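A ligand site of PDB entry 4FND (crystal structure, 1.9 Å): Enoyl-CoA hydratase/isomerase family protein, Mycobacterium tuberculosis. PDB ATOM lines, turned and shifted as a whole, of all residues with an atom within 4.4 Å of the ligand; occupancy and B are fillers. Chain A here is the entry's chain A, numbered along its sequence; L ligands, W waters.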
ATOM      1  N   LYS A  23       0.437   9.425  -1.494  1.00  0.00           N
ATOM      2  CA  LYS A  23      -0.634   9.951  -0.663  1.00  0.00           C
ATOM      3  C   LYS A  23      -1.136   8.885   0.305  1.00  0.00           C
ATOM      4  O   LYS A  23      -0.377   8.402   1.146  1.00  0.00           O
ATOM      5  CB  LYS A  23      -1.764  10.500  -1.552  1.00  0.00           C
ATOM      6  CG  LYS A  23      -2.468  11.723  -1.010  1.00  0.00           C
ATOM      7  CD  LYS A  23      -2.997  12.571  -2.149  1.00  0.00           C
ATOM      8  CE  LYS A  23      -3.829  13.746  -1.650  1.00  0.00           C
ATOM      9  N   VAL A  24      -2.409   8.506   0.176  1.00  0.00           N
ATOM     10  CA  VAL A  24      -2.979   7.528   1.102  1.00  0.00           C
ATOM     11  C   VAL A  24      -3.324   6.181   0.428  1.00  0.00           C
ATOM     12  O   VAL A  24      -4.214   5.463   0.886  1.00  0.00           O
ATOM     13  CB  VAL A  24      -4.208   8.081   1.846  1.00  0.00           C
ATOM     14  CG1 VAL A  24      -3.812   9.262   2.715  1.00  0.00           C
ATOM     15  CG2 VAL A  24      -5.311   8.491   0.857  1.00  0.00           C
ATOM     16  N   ALA A  26      -4.954   5.229  -2.186  1.00  0.00           N
ATOM     17  CA  ALA A  26      -6.345   5.038  -2.592  1.00  0.00           C
ATOM     18  C   ALA A  26      -6.448   3.896  -3.608  1.00  0.00           C
ATOM     19  O   ALA A  26      -5.662   3.821  -4.547  1.00  0.00           O
ATOM     20  CB  ALA A  26      -6.915   6.330  -3.166  1.00  0.00           C
ATOM     21  N   ARG A  57       2.879   6.378   5.543  1.00  0.00           N
ATOM     22  CA  ARG A  57       1.740   7.142   6.034  1.00  0.00           C
ATOM     23  C   ARG A  57       0.540   6.244   6.353  1.00  0.00           C
ATOM     24  O   ARG A  57      -0.102   6.400   7.394  1.00  0.00           O
ATOM     25  CB  ARG A  57       1.344   8.183   4.986  1.00  0.00           C
ATOM     26  CG  ARG A  57       0.368   9.265   5.453  1.00  0.00           C
ATOM     27  CD  ARG A  57       0.362  10.418   4.455  1.00  0.00           C
ATOM     28  NE  ARG A  57       1.714  10.890   4.194  1.00  0.00           N
ATOM     29  CZ  ARG A  57       2.061  11.740   3.229  1.00  0.00           C
ATOM     30  NH1 ARG A  57       3.328  12.104   3.083  1.00  0.00           N
ATOM     31  NH2 ARG A  57       1.133  12.228   2.417  1.00  0.00           N
ATOM     32  N   VAL A  58       0.233   5.306   5.457  1.00  0.00           N
ATOM     33  CA  VAL A  58      -0.880   4.405   5.678  1.00  0.00           C
ATOM     34  C   VAL A  58      -0.602   3.044   5.106  1.00  0.00           C
ATOM     35  O   VAL A  58       0.339   2.874   4.324  1.00  0.00           O
ATOM     36  CB  VAL A  58      -2.161   4.909   4.965  1.00  0.00           C
ATOM     37  CG1 VAL A  58      -2.612   6.235   5.547  1.00  0.00           C
ATOM     38  CG2 VAL A  58      -1.922   4.998   3.443  1.00  0.00           C
ATOM     39  N   GLY A  61      -6.034   4.139   2.630  1.00  0.00           N
ATOM     40  CA  GLY A  61      -7.223   4.833   3.042  1.00  0.00           C
ATOM     41  C   GLY A  61      -8.481   4.326   2.347  1.00  0.00           C
ATOM     42  O   GLY A  61      -9.554   4.909   2.524  1.00  0.00           O
ATOM     43  N   PHE A  63     -10.997   2.881  -0.899  1.00  0.00           N
ATOM     44  CA  PHE A  63     -11.342   3.285  -2.259  1.00  0.00           C
ATOM     45  C   PHE A  63     -11.120   4.781  -2.477  1.00  0.00           C
ATOM     46  O   PHE A  63     -11.213   5.576  -1.541  1.00  0.00           O
ATOM     47  CB  PHE A  63     -12.800   2.944  -2.561  1.00  0.00           C
ATOM     48  CG  PHE A  63     -13.059   1.481  -2.751  1.00  0.00           C
ATOM     49  CD1 PHE A  63     -12.408   0.776  -3.762  1.00  0.00           C
ATOM     50  CD2 PHE A  63     -13.964   0.804  -1.952  1.00  0.00           C
ATOM     51  CE1 PHE A  63     -12.640  -0.572  -3.954  1.00  0.00           C
ATOM     52  CE2 PHE A  63     -14.217  -0.547  -2.136  1.00  0.00           C
ATOM     53  CZ  PHE A  63     -13.555  -1.236  -3.137  1.00  0.00           C
ATOM     54  N   ASP A  64     -10.854   5.159  -3.732  1.00  0.00           N
ATOM     55  CA  ASP A  64     -10.729   6.559  -4.117  1.00  0.00           C
ATOM     56  C   ASP A  64     -12.059   7.280  -3.960  1.00  0.00           C
ATOM     57  O   ASP A  64     -13.010   7.016  -4.704  1.00  0.00           O
ATOM     58  CB  ASP A  64     -10.256   6.656  -5.573  1.00  0.00           C
ATOM     59  CG  ASP A  64      -9.931   8.067  -5.997  1.00  0.00           C
ATOM     60  OD1 ASP A  64     -10.255   9.021  -5.255  1.00  0.00           O
ATOM     61  OD2 ASP A  64      -9.342   8.218  -7.081  1.00  0.00           O
ATOM     62  N   LEU A  65     -12.107   8.211  -3.010  1.00  0.00           N
ATOM     63  CA  LEU A  65     -13.314   8.985  -2.715  1.00  0.00           C
ATOM     64  C   LEU A  65     -13.721   9.920  -3.859  1.00  0.00           C
ATOM     65  O   LEU A  65     -14.905  10.249  -4.006  1.00  0.00           O
ATOM     66  CB  LEU A  65     -13.115   9.829  -1.444  1.00  0.00           C
ATOM     67  CG  LEU A  65     -13.137   9.129  -0.082  1.00  0.00           C
ATOM     68  CD1 LEU A  65     -12.802  10.126   1.027  1.00  0.00           C
ATOM     69  CD2 LEU A  65     -14.486   8.479   0.156  1.00  0.00           C
ATOM     70  N   LEU A  68     -15.654   7.627  -6.126  1.00  0.00           N
ATOM     71  CA  LEU A  68     -16.827   7.178  -5.401  1.00  0.00           C
ATOM     72  C   LEU A  68     -17.937   8.234  -5.380  1.00  0.00           C
ATOM     73  O   LEU A  68     -19.113   7.904  -5.541  1.00  0.00           O
ATOM     74  CB  LEU A  68     -16.450   6.772  -3.965  1.00  0.00           C
ATOM     75  CG  LEU A  68     -17.547   6.076  -3.161  1.00  0.00           C
ATOM     76  CD1 LEU A  68     -17.881   4.726  -3.782  1.00  0.00           C
ATOM     77  CD2 LEU A  68     -17.124   5.914  -1.710  1.00  0.00           C
ATOM     78  N   LEU A  80     -15.568  -0.444  -7.178  1.00  0.00           N
ATOM     79  CA  LEU A  80     -15.948  -1.322  -6.089  1.00  0.00           C
ATOM     80  C   LEU A  80     -15.818  -2.790  -6.482  1.00  0.00           C
ATOM     81  O   LEU A  80     -15.238  -3.576  -5.733  1.00  0.00           O
ATOM     82  CB  LEU A  80     -17.364  -1.003  -5.602  1.00  0.00           C
ATOM     83  CG  LEU A  80     -17.512  -0.122  -4.355  1.00  0.00           C
ATOM     84  CD1 LEU A  80     -16.540   1.060  -4.367  1.00  0.00           C
ATOM     85  CD2 LEU A  80     -18.938   0.379  -4.236  1.00  0.00           C
ATOM     86  N   HIS A 104      -2.256   3.469   8.859  1.00  0.00           N
ATOM     87  CA  HIS A 104      -3.669   3.222   9.099  1.00  0.00           C
ATOM     88  C   HIS A 104      -4.296   2.435   7.949  1.00  0.00           C
ATOM     89  O   HIS A 104      -3.836   2.511   6.808  1.00  0.00           O
ATOM     90  CB  HIS A 104      -4.416   4.538   9.298  1.00  0.00           C
ATOM     91  CG  HIS A 104      -3.771   5.458  10.294  1.00  0.00           C
ATOM     92  ND1 HIS A 104      -3.547   5.091  11.602  1.00  0.00           N
ATOM     93  CD2 HIS A 104      -3.309   6.727  10.179  1.00  0.00           C
ATOM     94  CE1 HIS A 104      -2.973   6.093  12.242  1.00  0.00           C
ATOM     95  NE2 HIS A 104      -2.814   7.089  11.398  1.00  0.00           N
ATOM     96  N   ILE A 106      -8.173   1.965   6.544  1.00  0.00           N
ATOM     97  CA  ILE A 106      -9.550   2.397   6.714  1.00  0.00           C
ATOM     98  C   ILE A 106     -10.437   1.817   5.598  1.00  0.00           C
ATOM     99  O   ILE A 106     -10.033   1.799   4.444  1.00  0.00           O
ATOM    100  CB  ILE A 106      -9.644   3.918   6.661  1.00  0.00           C
ATOM    101  CG1 ILE A 106      -8.669   4.566   7.665  1.00  0.00           C
ATOM    102  CG2 ILE A 106     -11.072   4.362   6.920  1.00  0.00           C
ATOM    103  CD1 ILE A 106      -8.963   4.237   9.118  1.00  0.00           C
ATOM    104  N   ALA A 107     -11.626   1.352   5.952  1.00  0.00           N
ATOM    105  CA  ALA A 107     -12.601   0.870   4.960  1.00  0.00           C
ATOM    106  C   ALA A 107     -12.009  -0.200   4.048  1.00  0.00           C
ATOM    107  O   ALA A 107     -11.574  -1.249   4.512  1.00  0.00           O
ATOM    108  CB  ALA A 107     -13.150   2.025   4.154  1.00  0.00           C
ATOM    109  N   PHE A 111     -10.331  -3.865   4.557  1.00  0.00           N
ATOM    110  CA  PHE A 111     -10.856  -5.101   3.955  1.00  0.00           C
ATOM    111  C   PHE A 111      -9.718  -5.806   3.220  1.00  0.00           C
ATOM    112  O   PHE A 111      -9.560  -7.019   3.307  1.00  0.00           O
ATOM    113  CB  PHE A 111     -12.047  -4.819   3.020  1.00  0.00           C
ATOM    114  CG  PHE A 111     -13.098  -3.956   3.656  1.00  0.00           C
ATOM    115  CD1 PHE A 111     -13.320  -4.020   5.024  1.00  0.00           C
ATOM    116  CD2 PHE A 111     -13.859  -3.069   2.908  1.00  0.00           C
ATOM    117  CE1 PHE A 111     -14.266  -3.221   5.638  1.00  0.00           C
ATOM    118  CE2 PHE A 111     -14.808  -2.261   3.519  1.00  0.00           C
ATOM    119  CZ  PHE A 111     -15.013  -2.334   4.876  1.00  0.00           C
ATOM    120  N   ASN A 130     -15.055   2.486   8.533  1.00  0.00           N
ATOM    121  CA  ASN A 130     -15.690   3.717   9.002  1.00  0.00           C
ATOM    122  C   ASN A 130     -16.977   4.052   8.269  1.00  0.00           C
ATOM    123  O   ASN A 130     -17.550   5.128   8.475  1.00  0.00           O
ATOM    124  CB  ASN A 130     -14.719   4.891   8.890  1.00  0.00           C
ATOM    125  CG  ASN A 130     -14.454   5.301   7.449  1.00  0.00           C
ATOM    126  OD1 ASN A 130     -14.434   4.455   6.554  1.00  0.00           O
ATOM    127  ND2 ASN A 130     -14.258   6.593   7.221  1.00  0.00           N
ATOM    128  N   GLU A 131     -17.443   3.140   7.425  1.00  0.00           N
ATOM    129  CA  GLU A 131     -18.641   3.380   6.612  1.00  0.00           C
ATOM    130  C   GLU A 131     -19.798   3.999   7.400  1.00  0.00           C
ATOM    131  O   GLU A 131     -20.323   5.039   7.030  1.00  0.00           O
ATOM    132  CB  GLU A 131     -19.100   2.076   5.936  1.00  0.00           C
ATOM    133  CG  GLU A 131     -18.282   1.705   4.691  1.00  0.00           C
ATOM    134  CD  GLU A 131     -16.923   1.073   5.003  1.00  0.00           C
ATOM    135  OE1 GLU A 131     -16.538   0.963   6.187  1.00  0.00           O
ATOM    136  OE2 GLU A 131     -16.223   0.686   4.037  1.00  0.00           O
ATOM    137  N   ILE A 134     -19.573   7.576   8.299  1.00  0.00           N
ATOM    138  CA  ILE A 134     -19.734   8.558   7.233  1.00  0.00           C
ATOM    139  C   ILE A 134     -20.998   8.332   6.401  1.00  0.00           C
ATOM    140  O   ILE A 134     -21.117   8.852   5.296  1.00  0.00           O
ATOM    141  CB  ILE A 134     -18.507   8.616   6.296  1.00  0.00           C
ATOM    142  CG1 ILE A 134     -18.277   7.259   5.633  1.00  0.00           C
ATOM    143  CG2 ILE A 134     -17.257   9.079   7.069  1.00  0.00           C
ATOM    144  CD1 ILE A 134     -17.250   7.302   4.538  1.00  0.00           C
ATOM    145  N   MET A 136     -22.536   5.411   5.192  1.00  0.00           N
ATOM    146  CA  MET A 136     -22.682   4.347   4.190  1.00  0.00           C
ATOM    147  C   MET A 136     -22.920   2.995   4.844  1.00  0.00           C
ATOM    148  O   MET A 136     -22.434   2.717   5.947  1.00  0.00           O
ATOM    149  CB  MET A 136     -21.472   4.303   3.251  1.00  0.00           C
ATOM    150  CG  MET A 136     -21.438   5.475   2.280  1.00  0.00           C
ATOM    151  SD  MET A 136     -20.192   5.358   0.981  1.00  0.00           S
ATOM    152  CE  MET A 136     -18.861   6.331   1.689  1.00  0.00           C
ATOM    153  N   PRO A 139     -20.936  -2.973   2.319  1.00  0.00           N
ATOM    154  CA  PRO A 139     -21.286  -3.936   1.266  1.00  0.00           C
ATOM    155  C   PRO A 139     -21.157  -5.367   1.780  1.00  0.00           C
ATOM    156  O   PRO A 139     -20.329  -5.640   2.646  1.00  0.00           O
ATOM    157  CB  PRO A 139     -20.226  -3.685   0.188  1.00  0.00           C
ATOM    158  CG  PRO A 139     -19.719  -2.313   0.457  1.00  0.00           C
ATOM    159  CD  PRO A 139     -19.809  -2.117   1.927  1.00  0.00           C
HETATM  160  C1  LIG L   1     -16.107   3.448   1.001  1.00  0.00           C
HETATM  161  O1  LIG L   1     -15.070   4.113   0.336  1.00  0.00           O
HETATM  162  C2  LIG L   1     -15.774   1.980   1.196  1.00  0.00           C
HETATM  163  C3  LIG L   1     -16.658   0.889   0.657  1.00  0.00           C
HETATM  164  O2  LIG L   1     -17.427   0.310   1.662  1.00  0.00           O
HETATM  165  C4  LIG L   1     -17.577   1.392  -0.446  1.00  0.00           C
HETATM  166  C5  LIG L   1     -19.067   1.150  -0.299  1.00  0.00           C
HETATM  167  C6  LIG L   1     -19.993   2.285  -0.703  1.00  0.00           C
HETATM  168  N1  LIG L   1      -9.626   8.723  -1.422  1.00  0.00           N
HETATM  169  O3  LIG L   1      -5.580  14.758   5.748  1.00  0.00           O
HETATM  170  P1  LIG L   1      -5.814  13.294   5.456  1.00  0.00           P
HETATM  171  C7  LIG L   1      -6.905  12.354   0.730  1.00  0.00           C
HETATM  172  S1  LIG L   1     -16.445   4.307   2.541  1.00  0.00           S
HETATM  173  C8  LIG L   1      -8.996   9.776  -1.962  1.00  0.00           C
HETATM  174  O4  LIG L   1      -7.038  12.793   6.200  1.00  0.00           O
HETATM  175  P2  LIG L   1      -4.238  11.743   7.259  1.00  0.00           P
HETATM  176  C9  LIG L   1      -7.348  13.648   1.307  1.00  0.00           C
HETATM  177  O5  LIG L   1      -8.300  14.251   0.469  1.00  0.00           O
HETATM  178  C10 LIG L   1     -14.938   4.856   3.329  1.00  0.00           C
HETATM  179  N2  LIG L   1      -8.305  10.657  -1.218  1.00  0.00           N
HETATM  180  O6  LIG L   1      -4.468  12.475   5.841  1.00  0.00           O
HETATM  181  C11 LIG L   1      -6.137  14.416   1.384  1.00  0.00           C
HETATM  182  O7  LIG L   1      -5.889  15.000   0.151  1.00  0.00           O
HETATM  183  P3  LIG L   1      -5.292  16.423   0.028  1.00  0.00           P
HETATM  184  C12 LIG L   1     -14.458   6.248   2.990  1.00  0.00           C
HETATM  185  C13 LIG L   1      -8.250  10.488   0.117  1.00  0.00           C
HETATM  186  O8  LIG L   1      -2.841  11.141   7.226  1.00  0.00           O
HETATM  187  C14 LIG L   1      -5.068  13.410   1.648  1.00  0.00           C
HETATM  188  O9  LIG L   1      -5.469  12.233   1.057  1.00  0.00           O
HETATM  189  N3  LIG L   1     -13.164   6.732   3.494  1.00  0.00           N
HETATM  190  C15 LIG L   1      -8.876   9.401   0.718  1.00  0.00           C
HETATM  191  O10 LIG L   1      -4.438  12.668   8.411  1.00  0.00           O
HETATM  192  C16 LIG L   1      -4.876  13.182   3.093  1.00  0.00           C
HETATM  193  O11 LIG L   1      -6.009  13.141   3.926  1.00  0.00           O
HETATM  194  C17 LIG L   1     -13.136   7.798   4.506  1.00  0.00           C
HETATM  195  O12 LIG L   1     -14.192   8.299   4.941  1.00  0.00           O
HETATM  196  C18 LIG L   1      -9.577   8.519  -0.093  1.00  0.00           C
HETATM  197  N4  LIG L   1     -10.262   7.354   0.521  1.00  0.00           N
HETATM  198  O13 LIG L   1      -5.224  10.539   7.357  1.00  0.00           O
HETATM  199  C19 LIG L   1     -11.851   8.321   5.043  1.00  0.00           C
HETATM  200  N5  LIG L   1      -8.645   9.476   2.058  1.00  0.00           N
HETATM  201  O14 LIG L   1      -5.583  17.154   1.304  1.00  0.00           O
HETATM  202  C20 LIG L   1     -10.589   7.692   4.491  1.00  0.00           C
HETATM  203  C21 LIG L   1      -7.894  10.561   2.293  1.00  0.00           C
HETATM  204  O15 LIG L   1      -3.803  16.289  -0.074  1.00  0.00           O
HETATM  205  N6  LIG L   1      -9.440   8.471   4.775  1.00  0.00           N
HETATM  206  N7  LIG L   1      -7.663  11.160   1.128  1.00  0.00           N
HETATM  207  O16 LIG L   1      -5.859  17.156  -1.176  1.00  0.00           O
HETATM  208  C22 LIG L   1      -8.955   8.584   6.115  1.00  0.00           C
HETATM  209  O17 LIG L   1      -9.500   8.007   7.062  1.00  0.00           O
HETATM  210  C23 LIG L   1      -7.714   9.429   6.391  1.00  0.00           C
HETATM  211  O18 LIG L   1      -7.571  10.377   5.362  1.00  0.00           O
HETATM  212  C24 LIG L   1      -6.430   8.614   6.516  1.00  0.00           C
HETATM  213  C25 LIG L   1      -5.258   9.583   6.395  1.00  0.00           C
HETATM  214  C26 LIG L   1      -6.398   7.592   5.450  1.00  0.00           C
HETATM  215  C27 LIG L   1      -6.352   7.949   7.865  1.00  0.00           C
HETATM  216  O   HOH W   1     -12.166   4.893   1.623  1.00  0.00           O
HETATM  217  O   HOH W   2      -9.078   7.869  10.158  1.00  0.00           O
HETATM  218  O   HOH W   3     -13.004   2.362   1.017  1.00  0.00           O
HETATM  219  O   HOH W   4     -13.613  10.560   6.126  1.00  0.00           O
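Lys 23 touches the ligand (CE to O15, 3.0 Å).
CG2 of Val 24 touches N7 of the ligand, at 3.6 Å.
Asp 64 touches the ligand (OD1 to C8, 3.6 Å).
Leu 68 touches the ligand (CD2 to O1, 3.4 Å).
Ile 106 touches the ligand.
Ala 107 touches the ligand (CB to C10, 3.4 Å).
Ile 134 touches the ligand.
CE of Met 136 touches S1 of the ligand (3.3 Å).
Pro 139 touches the ligand.
Hydrophobic or aromatic side chains within 4 Å of the ligand: Val 24, Phe 63, Leu 65, Leu 68, Ile 106, Ala 107, Ile 134, Met 136 and Pro 139.
14 residues have an atom within 4 Å of the ligand: Lys 23, Val 24, Gly 61, Phe 63, Asp 64, Leu 65, Leu 68, Ile 106, Ala 107, Asn 130, Glu 131, Ile 134, Met 136 and Pro 139.
N of Met 136 lies within hydrogen-bond range of O of Glu 131.
The backbone NH of Gly 61 lies within hydrogen-bond range of the backbone carbonyl oxygen of Val 24 (2.8 Å).
OE2 of Glu 131 is in hydrogen-bond range of O2 of the ligand, at 2.7 Å.
An oxygen (O12) of the ligand sits at hydrogen-bond distance from the side-chain amide nitrogen (ND2) of Asn 130 (2.8 Å).
The backbone carbonyl oxygen (O) of Phe 63 lies within hydrogen-bond range of a nitrogen (N4) of the ligand, at 2.9 Å.
A nitrogen (N1) of the ligand is in hydrogen-bond range of the backbone NH of Leu 65, at 3.0 Å.
A nitrogen (N4) of the ligand is in hydrogen-bond range of the backbone carbonyl oxygen (O) of Gly 61 (3.2 Å).
Water W3 lies within hydrogen-bond range of O1 of the ligand (2.8 Å) and N of Phe 63 (2.8 Å).
Water W1 lies within hydrogen-bond range of O of Gly 61 (2.8 Å), N3 of the ligand (2.8 Å) and O of Phe 63 (3.4 Å).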
